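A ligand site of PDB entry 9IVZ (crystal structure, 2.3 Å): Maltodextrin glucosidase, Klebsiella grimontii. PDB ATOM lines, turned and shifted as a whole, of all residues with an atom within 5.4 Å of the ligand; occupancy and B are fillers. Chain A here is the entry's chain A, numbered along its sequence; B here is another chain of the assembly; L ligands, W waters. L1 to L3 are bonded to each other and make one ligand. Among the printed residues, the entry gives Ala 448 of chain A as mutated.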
ATOM      1  N   GLY A 170      10.571 -10.770  -1.993  1.00  0.00           N
ATOM      2  CA  GLY A 170      10.884  -9.836  -3.065  1.00  0.00           C
ATOM      3  C   GLY A 170      12.054 -10.249  -3.944  1.00  0.00           C
ATOM      4  O   GLY A 170      12.125  -9.855  -5.105  1.00  0.00           O
ATOM      5  N   GLY A 171      12.973 -11.043  -3.419  1.00  0.00           N
ATOM      6  CA  GLY A 171      14.111 -11.498  -4.179  1.00  0.00           C
ATOM      7  C   GLY A 171      13.970 -12.876  -4.751  1.00  0.00           C
ATOM      8  O   GLY A 171      14.892 -13.343  -5.441  1.00  0.00           O
ATOM      9  N   VAL A 208      16.046 -13.604  -7.993  1.00  0.00           N
ATOM     10  CA  VAL A 208      15.422 -13.126  -9.229  1.00  0.00           C
ATOM     11  C   VAL A 208      16.216 -11.973  -9.821  1.00  0.00           C
ATOM     12  O   VAL A 208      16.242 -11.804 -11.047  1.00  0.00           O
ATOM     13  CB  VAL A 208      13.962 -12.725  -8.966  1.00  0.00           C
ATOM     14  CG1 VAL A 208      13.889 -11.540  -7.985  1.00  0.00           C
ATOM     15  CG2 VAL A 208      13.254 -12.380 -10.267  1.00  0.00           C
ATOM     16  N   HIS A 209      16.880 -11.162  -9.001  1.00  0.00           N
ATOM     17  CA  HIS A 209      17.655 -10.040  -9.517  1.00  0.00           C
ATOM     18  C   HIS A 209      19.062 -10.447  -9.924  1.00  0.00           C
ATOM     19  O   HIS A 209      19.648  -9.829 -10.819  1.00  0.00           O
ATOM     20  CB  HIS A 209      17.688  -8.934  -8.472  1.00  0.00           C
ATOM     21  CG  HIS A 209      18.175  -9.391  -7.133  1.00  0.00           C
ATOM     22  ND1 HIS A 209      19.507  -9.668  -6.881  1.00  0.00           N
ATOM     23  CD2 HIS A 209      17.508  -9.682  -6.000  1.00  0.00           C
ATOM     24  CE1 HIS A 209      19.630 -10.097  -5.643  1.00  0.00           C
ATOM     25  NE2 HIS A 209      18.437 -10.106  -5.076  1.00  0.00           N
ATOM     26  N   TYR A 211      22.060 -10.337  -8.464  1.00  0.00           N
ATOM     27  CA  TYR A 211      23.305  -9.710  -8.005  1.00  0.00           C
ATOM     28  C   TYR A 211      24.062 -10.615  -7.046  1.00  0.00           C
ATOM     29  O   TYR A 211      25.182 -10.283  -6.641  1.00  0.00           O
ATOM     30  CB  TYR A 211      23.026  -8.350  -7.355  1.00  0.00           C
ATOM     31  CG  TYR A 211      22.657  -7.280  -8.360  1.00  0.00           C
ATOM     32  CD1 TYR A 211      23.642  -6.661  -9.134  1.00  0.00           C
ATOM     33  CD2 TYR A 211      21.337  -6.907  -8.557  1.00  0.00           C
ATOM     34  CE1 TYR A 211      23.311  -5.682 -10.081  1.00  0.00           C
ATOM     35  CE2 TYR A 211      20.991  -5.950  -9.515  1.00  0.00           C
ATOM     36  CZ  TYR A 211      21.979  -5.345 -10.264  1.00  0.00           C
ATOM     37  OH  TYR A 211      21.610  -4.397 -11.207  1.00  0.00           O
ATOM     38  N   VAL A 248      28.960  -7.387 -11.828  1.00  0.00           N
ATOM     39  CA  VAL A 248      28.808  -7.408 -10.370  1.00  0.00           C
ATOM     40  C   VAL A 248      30.093  -7.932  -9.729  1.00  0.00           C
ATOM     41  O   VAL A 248      30.190  -9.105  -9.388  1.00  0.00           O
ATOM     42  CB  VAL A 248      27.593  -8.251  -9.956  1.00  0.00           C
ATOM     43  CG1 VAL A 248      27.213  -7.976  -8.487  1.00  0.00           C
ATOM     44  CG2 VAL A 248      26.412  -7.960 -10.890  1.00  0.00           C
ATOM     45  N   HIS A 251      31.273  -7.936  -5.131  1.00  0.00           N
ATOM     46  CA  HIS A 251      30.863  -9.001  -4.244  1.00  0.00           C
ATOM     47  C   HIS A 251      30.338 -10.146  -5.101  1.00  0.00           C
ATOM     48  O   HIS A 251      29.873  -9.924  -6.216  1.00  0.00           O
ATOM     49  CB  HIS A 251      29.782  -8.507  -3.281  1.00  0.00           C
ATOM     50  CG  HIS A 251      28.518  -8.127  -3.982  1.00  0.00           C
ATOM     51  ND1 HIS A 251      28.175  -6.825  -4.267  1.00  0.00           N
ATOM     52  CD2 HIS A 251      27.531  -8.894  -4.513  1.00  0.00           C
ATOM     53  CE1 HIS A 251      27.021  -6.797  -4.904  1.00  0.00           C
ATOM     54  NE2 HIS A 251      26.612  -8.046  -5.073  1.00  0.00           N
ATOM     55  N   TRP A 292      28.710  -8.793   4.455  1.00  0.00           N
ATOM     56  CA  TRP A 292      28.971  -7.490   3.838  1.00  0.00           C
ATOM     57  C   TRP A 292      27.753  -6.610   4.065  1.00  0.00           C
ATOM     58  O   TRP A 292      26.639  -6.978   3.688  1.00  0.00           O
ATOM     59  CB  TRP A 292      29.284  -7.595   2.345  1.00  0.00           C
ATOM     60  CG  TRP A 292      29.495  -6.221   1.750  1.00  0.00           C
ATOM     61  CD1 TRP A 292      30.396  -5.276   2.173  1.00  0.00           C
ATOM     62  CD2 TRP A 292      28.793  -5.630   0.647  1.00  0.00           C
ATOM     63  NE1 TRP A 292      30.285  -4.131   1.407  1.00  0.00           N
ATOM     64  CE2 TRP A 292      29.321  -4.325   0.463  1.00  0.00           C
ATOM     65  CE3 TRP A 292      27.775  -6.066  -0.216  1.00  0.00           C
ATOM     66  CZ2 TRP A 292      28.853  -3.471  -0.545  1.00  0.00           C
ATOM     67  CZ3 TRP A 292      27.325  -5.219  -1.199  1.00  0.00           C
ATOM     68  CH2 TRP A 292      27.865  -3.933  -1.361  1.00  0.00           C
ATOM     69  N   LEU A 293      27.983  -5.441   4.646  1.00  0.00           N
ATOM     70  CA  LEU A 293      26.889  -4.586   5.112  1.00  0.00           C
ATOM     71  C   LEU A 293      25.911  -5.470   5.881  1.00  0.00           C
ATOM     72  O   LEU A 293      26.306  -6.155   6.823  1.00  0.00           O
ATOM     73  CB  LEU A 293      26.210  -3.856   3.954  1.00  0.00           C
ATOM     74  CG  LEU A 293      27.140  -2.908   3.161  1.00  0.00           C
ATOM     75  CD1 LEU A 293      26.351  -1.932   2.297  1.00  0.00           C
ATOM     76  CD2 LEU A 293      28.131  -2.162   4.041  1.00  0.00           C
ATOM     77  N   TYR A 295      24.379  -8.083   4.529  1.00  0.00           N
ATOM     78  CA  TYR A 295      24.070  -9.216   3.660  1.00  0.00           C
ATOM     79  C   TYR A 295      24.965 -10.402   3.948  1.00  0.00           C
ATOM     80  O   TYR A 295      26.184 -10.344   3.725  1.00  0.00           O
ATOM     81  CB  TYR A 295      24.219  -8.815   2.190  1.00  0.00           C
ATOM     82  CG  TYR A 295      23.374  -7.647   1.787  1.00  0.00           C
ATOM     83  CD1 TYR A 295      22.002  -7.799   1.615  1.00  0.00           C
ATOM     84  CD2 TYR A 295      23.950  -6.399   1.556  1.00  0.00           C
ATOM     85  CE1 TYR A 295      21.204  -6.734   1.221  1.00  0.00           C
ATOM     86  CE2 TYR A 295      23.160  -5.324   1.166  1.00  0.00           C
ATOM     87  CZ  TYR A 295      21.781  -5.493   1.003  1.00  0.00           C
ATOM     88  OH  TYR A 295      20.977  -4.446   0.615  1.00  0.00           O
ATOM     89  N   SER A 297      24.127 -12.888   2.038  1.00  0.00           N
ATOM     90  CA  SER A 297      24.077 -13.444   0.686  1.00  0.00           C
ATOM     91  C   SER A 297      25.122 -12.854  -0.251  1.00  0.00           C
ATOM     92  O   SER A 297      25.393 -13.463  -1.290  1.00  0.00           O
ATOM     93  CB  SER A 297      22.685 -13.254   0.082  1.00  0.00           C
ATOM     94  OG  SER A 297      22.321 -11.890   0.072  1.00  0.00           O
ATOM     95  N   LEU A 298      25.713 -11.707   0.073  1.00  0.00           N
ATOM     96  CA  LEU A 298      26.555 -10.955  -0.860  1.00  0.00           C
ATOM     97  C   LEU A 298      27.947 -10.688  -0.298  1.00  0.00           C
ATOM     98  O   LEU A 298      28.354  -9.531  -0.165  1.00  0.00           O
ATOM     99  CB  LEU A 298      25.886  -9.640  -1.251  1.00  0.00           C
ATOM    100  CG  LEU A 298      24.438  -9.647  -1.748  1.00  0.00           C
ATOM    101  CD1 LEU A 298      23.873  -8.259  -1.840  1.00  0.00           C
ATOM    102  CD2 LEU A 298      24.355 -10.338  -3.099  1.00  0.00           C
ATOM    103  N   ASP A 336      28.306  -2.669 -11.211  1.00  0.00           N
ATOM    104  CA  ASP A 336      27.497  -2.598 -10.000  1.00  0.00           C
ATOM    105  C   ASP A 336      28.375  -2.272  -8.797  1.00  0.00           C
ATOM    106  O   ASP A 336      29.509  -2.743  -8.721  1.00  0.00           O
ATOM    107  CB  ASP A 336      26.780  -3.926  -9.781  1.00  0.00           C
ATOM    108  CG  ASP A 336      25.888  -3.919  -8.547  1.00  0.00           C
ATOM    109  OD1 ASP A 336      24.982  -3.073  -8.479  1.00  0.00           O
ATOM    110  OD2 ASP A 336      26.088  -4.760  -7.652  1.00  0.00           O
ATOM    111  N   VAL A 337      27.843  -1.471  -7.869  1.00  0.00           N
ATOM    112  CA  VAL A 337      28.558  -1.020  -6.663  1.00  0.00           C
ATOM    113  C   VAL A 337      29.967  -0.595  -7.021  1.00  0.00           C
ATOM    114  O   VAL A 337      30.941  -1.077  -6.431  1.00  0.00           O
ATOM    115  CB  VAL A 337      28.570  -2.127  -5.576  1.00  0.00           C
ATOM    116  CG1 VAL A 337      28.963  -1.539  -4.217  1.00  0.00           C
ATOM    117  CG2 VAL A 337      27.236  -2.828  -5.476  1.00  0.00           C
ATOM    118  N   HIS A 339      31.597   2.111  -6.571  1.00  0.00           N
ATOM    119  CA  HIS A 339      32.256   2.997  -5.626  1.00  0.00           C
ATOM    120  C   HIS A 339      32.759   2.287  -4.368  1.00  0.00           C
ATOM    121  O   HIS A 339      33.512   2.891  -3.596  1.00  0.00           O
ATOM    122  CB  HIS A 339      31.284   4.107  -5.235  1.00  0.00           C
ATOM    123  CG  HIS A 339      30.067   3.607  -4.502  1.00  0.00           C
ATOM    124  ND1 HIS A 339      29.301   2.556  -4.962  1.00  0.00           N
ATOM    125  CD2 HIS A 339      29.505   4.007  -3.332  1.00  0.00           C
ATOM    126  CE1 HIS A 339      28.313   2.340  -4.113  1.00  0.00           C
ATOM    127  NE2 HIS A 339      28.415   3.199  -3.119  1.00  0.00           N
ATOM    128  N   MET A 340      32.362   1.043  -4.117  1.00  0.00           N
ATOM    129  CA  MET A 340      32.753   0.372  -2.888  1.00  0.00           C
ATOM    130  C   MET A 340      33.709  -0.790  -3.110  1.00  0.00           C
ATOM    131  O   MET A 340      34.320  -1.259  -2.146  1.00  0.00           O
ATOM    132  CB  MET A 340      31.525  -0.125  -2.127  1.00  0.00           C
ATOM    133  CG  MET A 340      30.531   0.984  -1.816  1.00  0.00           C
ATOM    134  SD  MET A 340      29.113   0.456  -0.843  1.00  0.00           S
ATOM    135  CE  MET A 340      29.863   0.328   0.781  1.00  0.00           C
ATOM    136  N   GLU A 373      27.530   2.471 -11.509  1.00  0.00           N
ATOM    137  CA  GLU A 373      26.358   2.981 -10.812  1.00  0.00           C
ATOM    138  C   GLU A 373      26.820   3.887  -9.674  1.00  0.00           C
ATOM    139  O   GLU A 373      27.400   3.414  -8.692  1.00  0.00           O
ATOM    140  CB  GLU A 373      25.509   1.837 -10.274  1.00  0.00           C
ATOM    141  CG  GLU A 373      24.369   2.315  -9.402  1.00  0.00           C
ATOM    142  CD  GLU A 373      23.685   1.185  -8.632  1.00  0.00           C
ATOM    143  OE1 GLU A 373      24.337   0.557  -7.747  1.00  0.00           O
ATOM    144  OE2 GLU A 373      22.484   0.934  -8.930  1.00  0.00           O
ATOM    145  N   PHE A 375      25.066   6.361  -7.213  1.00  0.00           N
ATOM    146  CA  PHE A 375      24.086   7.178  -6.488  1.00  0.00           C
ATOM    147  C   PHE A 375      24.717   8.457  -5.971  1.00  0.00           C
ATOM    148  O   PHE A 375      24.031   9.476  -5.816  1.00  0.00           O
ATOM    149  CB  PHE A 375      23.475   6.376  -5.344  1.00  0.00           C
ATOM    150  CG  PHE A 375      22.308   5.514  -5.759  1.00  0.00           C
ATOM    151  CD1 PHE A 375      22.512   4.397  -6.570  1.00  0.00           C
ATOM    152  CD2 PHE A 375      21.026   5.834  -5.376  1.00  0.00           C
ATOM    153  CE1 PHE A 375      21.439   3.596  -6.979  1.00  0.00           C
ATOM    154  CE2 PHE A 375      19.936   5.041  -5.778  1.00  0.00           C
ATOM    155  CZ  PHE A 375      20.153   3.922  -6.585  1.00  0.00           C
ATOM    156  N   HIS A 447      15.973  -0.020 -11.360  1.00  0.00           N
ATOM    157  CA  HIS A 447      15.628  -1.143 -10.506  1.00  0.00           C
ATOM    158  C   HIS A 447      15.920  -0.893  -9.033  1.00  0.00           C
ATOM    159  O   HIS A 447      15.508  -1.692  -8.190  1.00  0.00           O
ATOM    160  CB  HIS A 447      16.392  -2.375 -10.957  1.00  0.00           C
ATOM    161  CG  HIS A 447      17.862  -2.229 -10.802  1.00  0.00           C
ATOM    162  ND1 HIS A 447      18.599  -1.352 -11.569  1.00  0.00           N
ATOM    163  CD2 HIS A 447      18.739  -2.804  -9.933  1.00  0.00           C
ATOM    164  CE1 HIS A 447      19.878  -1.406 -11.200  1.00  0.00           C
ATOM    165  NE2 HIS A 447      19.981  -2.279 -10.212  1.00  0.00           N
ATOM    166  N   ALA A 448      16.662   0.179  -8.714  1.00  0.00           N
ATOM    167  CA  ALA A 448      17.083   0.496  -7.358  1.00  0.00           C
ATOM    168  C   ALA A 448      16.418   1.753  -6.815  1.00  0.00           C
ATOM    169  O   ALA A 448      16.807   2.240  -5.743  1.00  0.00           O
ATOM    170  CB  ALA A 448      18.605   0.632  -7.297  1.00  0.00           C
ATOM    171  N   ASP A 492      11.946  -0.818  -4.836  1.00  0.00           N
ATOM    172  CA  ASP A 492      12.331  -2.218  -4.703  1.00  0.00           C
ATOM    173  C   ASP A 492      11.661  -2.847  -3.483  1.00  0.00           C
ATOM    174  O   ASP A 492      11.938  -2.443  -2.346  1.00  0.00           O
ATOM    175  CB  ASP A 492      13.857  -2.272  -4.603  1.00  0.00           C
ATOM    176  CG  ASP A 492      14.395  -3.671  -4.563  1.00  0.00           C
ATOM    177  OD1 ASP A 492      13.653  -4.613  -4.898  1.00  0.00           O
ATOM    178  OD2 ASP A 492      15.585  -3.829  -4.193  1.00  0.00           O
ATOM    179  N   PRO A 493      10.801  -3.859  -3.671  1.00  0.00           N
ATOM    180  CA  PRO A 493      10.527  -4.635  -4.891  1.00  0.00           C
ATOM    181  C   PRO A 493       9.538  -4.038  -5.913  1.00  0.00           C
ATOM    182  O   PRO A 493       9.489  -4.547  -7.033  1.00  0.00           O
ATOM    183  CB  PRO A 493       9.961  -5.932  -4.321  1.00  0.00           C
ATOM    184  CG  PRO A 493       9.194  -5.478  -3.134  1.00  0.00           C
ATOM    185  CD  PRO A 493      10.064  -4.400  -2.516  1.00  0.00           C
ATOM    186  N   ARG A 496       9.818  -3.098  -9.944  1.00  0.00           N
ATOM    187  CA  ARG A 496      10.120  -4.160 -10.901  1.00  0.00           C
ATOM    188  C   ARG A 496       8.850  -4.888 -11.325  1.00  0.00           C
ATOM    189  O   ARG A 496       8.818  -6.122 -11.386  1.00  0.00           O
ATOM    190  CB  ARG A 496      11.139  -5.127 -10.299  1.00  0.00           C
ATOM    191  CG  ARG A 496      12.395  -4.427  -9.816  1.00  0.00           C
ATOM    192  CD  ARG A 496      13.173  -5.240  -8.808  1.00  0.00           C
ATOM    193  NE  ARG A 496      14.269  -4.429  -8.299  1.00  0.00           N
ATOM    194  CZ  ARG A 496      15.336  -4.904  -7.667  1.00  0.00           C
ATOM    195  NH1 ARG A 496      15.466  -6.201  -7.409  1.00  0.00           N
ATOM    196  NH2 ARG A 496      16.294  -4.057  -7.300  1.00  0.00           N
ATOM    197  N   GLU B  44      30.034   5.179   0.261  1.00  0.00           N
ATOM    198  CA  GLU B  44      28.574   5.138   0.262  1.00  0.00           C
ATOM    199  C   GLU B  44      28.030   6.261   1.138  1.00  0.00           C
ATOM    200  O   GLU B  44      28.504   6.477   2.258  1.00  0.00           O
ATOM    201  CB  GLU B  44      28.069   3.789   0.754  1.00  0.00           C
ATOM    202  CG  GLU B  44      26.564   3.722   0.992  1.00  0.00           C
ATOM    203  CD  GLU B  44      25.767   3.573  -0.293  1.00  0.00           C
ATOM    204  OE1 GLU B  44      26.278   3.954  -1.362  1.00  0.00           O
ATOM    205  OE2 GLU B  44      24.621   3.078  -0.222  1.00  0.00           O
HETATM  206  C1  LIG L   1      22.653   2.674  -3.066  1.00  0.00           C
HETATM  207  C2  LIG L   1      24.003   2.008  -3.294  1.00  0.00           C
HETATM  208  C3  LIG L   1      23.966   0.930  -4.355  1.00  0.00           C
HETATM  209  C4  LIG L   1      22.600   0.285  -4.596  1.00  0.00           C
HETATM  210  C5  LIG L   1      21.388   0.764  -3.755  1.00  0.00           C
HETATM  211  C6  LIG L   1      20.435  -0.315  -3.371  1.00  0.00           C
HETATM  212  O1  LIG L   1      22.754   3.708  -2.087  1.00  0.00           O
HETATM  213  O2  LIG L   1      24.940   3.027  -3.644  1.00  0.00           O
HETATM  214  O3  LIG L   1      25.061   0.001  -4.159  1.00  0.00           O
HETATM  215  O4  LIG L   1      22.478  -1.107  -5.048  1.00  0.00           O
HETATM  216  O5  LIG L   1      21.714   1.646  -2.597  1.00  0.00           O
HETATM  217  O6  LIG L   1      20.483  -0.530  -2.001  1.00  0.00           O
HETATM  218  C1  LG2 L   2      23.103  -2.250  -4.544  1.00  0.00           C
HETATM  219  C2  LG2 L   2      22.967  -3.252  -5.673  1.00  0.00           C
HETATM  220  C3  LG2 L   2      23.120  -4.678  -5.318  1.00  0.00           C
HETATM  221  C4  LG2 L   2      22.444  -5.072  -4.055  1.00  0.00           C
HETATM  222  C5  LG2 L   2      22.641  -4.067  -2.924  1.00  0.00           C
HETATM  223  C6  LG2 L   2      24.051  -4.106  -2.293  1.00  0.00           C
HETATM  224  O1  LG2 L   2      21.637  -3.113  -6.322  1.00  0.00           O
HETATM  225  O2  LG2 L   2      24.549  -4.999  -5.294  1.00  0.00           O
HETATM  226  O3  LG2 L   2      20.962  -5.169  -4.295  1.00  0.00           O
HETATM  227  O4  LG2 L   2      22.377  -2.679  -3.327  1.00  0.00           O
HETATM  228  O5  LG2 L   2      24.090  -3.119  -1.260  1.00  0.00           O
HETATM  229  O1  LG3 L   3      20.540  -7.498  -3.842  1.00  0.00           O
HETATM  230  C1  LG3 L   3      19.056  -6.232  -5.311  1.00  0.00           C
HETATM  231  C2  LG3 L   3      18.091  -5.935  -4.204  1.00  0.00           C
HETATM  232  C3  LG3 L   3      15.152  -8.313  -2.748  1.00  0.00           C
HETATM  233  C4  LG3 L   3      14.542  -8.036   1.530  1.00  0.00           C
HETATM  234  C5  LG3 L   3      14.894  -7.628   0.078  1.00  0.00           C
HETATM  235  C6  LG3 L   3      16.280  -8.250  -0.490  1.00  0.00           C
HETATM  236  C7  LG3 L   3      16.600  -8.122  -1.876  1.00  0.00           C
HETATM  237  C8  LG3 L   3      18.417  -6.426  -2.807  1.00  0.00           C
HETATM  238  C9  LG3 L   3      19.808  -7.152  -2.582  1.00  0.00           C
HETATM  239  C10 LG3 L   3      19.892  -8.330  -1.668  1.00  0.00           C
HETATM  240  C11 LG3 L   3      20.499  -6.410  -4.829  1.00  0.00           C
HETATM  241  C12 LG3 L   3      14.361  -7.306  -2.488  1.00  0.00           C
HETATM  242  C13 LG3 L   3      13.815  -7.418  -0.859  1.00  0.00           C
HETATM  243  N1  LG3 L   3      17.137  -6.783  -2.025  1.00  0.00           N
HETATM  244  O2  LG3 L   3      13.518  -7.183   2.051  1.00  0.00           O
HETATM  245  O3  LG3 L   3      19.030  -5.114  -6.185  1.00  0.00           O
HETATM  246  O4  LG3 L   3      16.731  -6.257  -4.622  1.00  0.00           O
HETATM  247  O5  LG3 L   3      15.476  -8.420  -4.155  1.00  0.00           O
HETATM  248  O6  LG3 L   3      13.188  -7.255  -3.340  1.00  0.00           O
HETATM  249  O7  LG3 L   3      13.115  -6.259  -0.565  1.00  0.00           O
HETATM  250  O   HOH W   1      22.517  -2.188  -8.628  1.00  0.00           O
HETATM  251  O   HOH W   2      17.998  -5.242  -0.027  1.00  0.00           O
HETATM  252  O   HOH W   3      11.795  -5.826   3.804  1.00  0.00           O
HETATM  253  O   HOH W   4      26.158   3.830  -6.138  1.00  0.00           O
HETATM  254  O   HOH W   5      25.768  -0.953  -1.895  1.00  0.00           O
HETATM  255  O   HOH W   6      17.823  -2.015  -4.381  1.00  0.00           O
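NE2 of His 339 lies within hydrogen-bond range of OE1 of Glu 44 of chain B, at 2.9 Å. OD2 of Asp 492 is in salt-bridge range of NH2 of Arg 496, at 3.2 Å. A ring nitrogen (ND1) of His 209 is in hydrogen-bond range of the backbone NH of Tyr 211, 3.1 Å away. The guanidinium group (NH2) of Arg 496 is in hydrogen-bond range of the backbone carbonyl oxygen (O) of His 447, at 2.6 Å. The backbone carbonyl oxygen (O) of Tyr 211 lies within hydrogen-bond range of a ring nitrogen (NE2) of His 251, 3.1 Å away. O of Gly 171 lies within hydrogen-bond range of N of Val 208, at 2.8 Å. A ring nitrogen (NE2) of His 339 lies close to the side-chain sulfur (SD) of Met 340, at 3.6 Å. A ring nitrogen (NE2) of His 447 is in hydrogen-bond range of the side-chain hydroxyl (OH) of Tyr 211.
Merely in contact with the ligand: Gly 171, His 209, Tyr 211, His 251, Trp 292, Tyr 295, Leu 298, Val 337, His 339, Glu 373, Phe 375 and Pro 493. Hydrophobic or aromatic side chains that line the ligand: His 209, Tyr 211, His 251, Trp 292, Tyr 295, Leu 298, Val 337, His 339, Phe 375 and Pro 493. 17 residues have an atom within 4 Å of the ligand: Gly 170, Gly 171, His 209, Tyr 211, His 251, Trp 292, Tyr 295, Leu 298, Asp 336, Val 337, His 339, Glu 373, Phe 375, Asp 492, Pro 493, Arg 496 and Glu 44 of chain B.
The side-chain carboxylate of Glu 44 of chain B lies within hydrogen-bond range of an oxygen (O1) of LIG L1, at 2.7 Å. The side-chain carboxylate (OD2) of Asp 492 lies within salt-bridge range of a nitrogen (N1) of LG3 L3, 3.98 Å away. OD2 of Asp 336 is in hydrogen-bond range of O2 of LG2 L2 (2.8 Å). The guanidinium group (NH1) of Arg 496 is in hydrogen-bond range of an oxygen (O4) of LG3 L3. O of Gly 170 sits close to O6 of LG3 L3 (3.3 Å).
Water W5 lies within hydrogen-bond range of an oxygen (O3) of LIG L1 (2.6 Å) and the side-chain sulfur (SD) of Met 340 (3.8 Å). Water W1 lies within hydrogen-bond range of the side-chain carboxylate of Asp 336, an oxygen (O1) of LG2 L2, a ring nitrogen (NE2) of His 447 and the side-chain carboxylate of Glu 373. Water W2 lies within hydrogen-bond range of a nitrogen (N1) of LG3 L3 and the side-chain hydroxyl (OH) of Tyr 295. Water W4 lies within hydrogen-bond range of O of Glu 373 (2.9 Å), O2 of LIG L1 (2.9 Å) and N of Phe 375 (3.0 Å).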
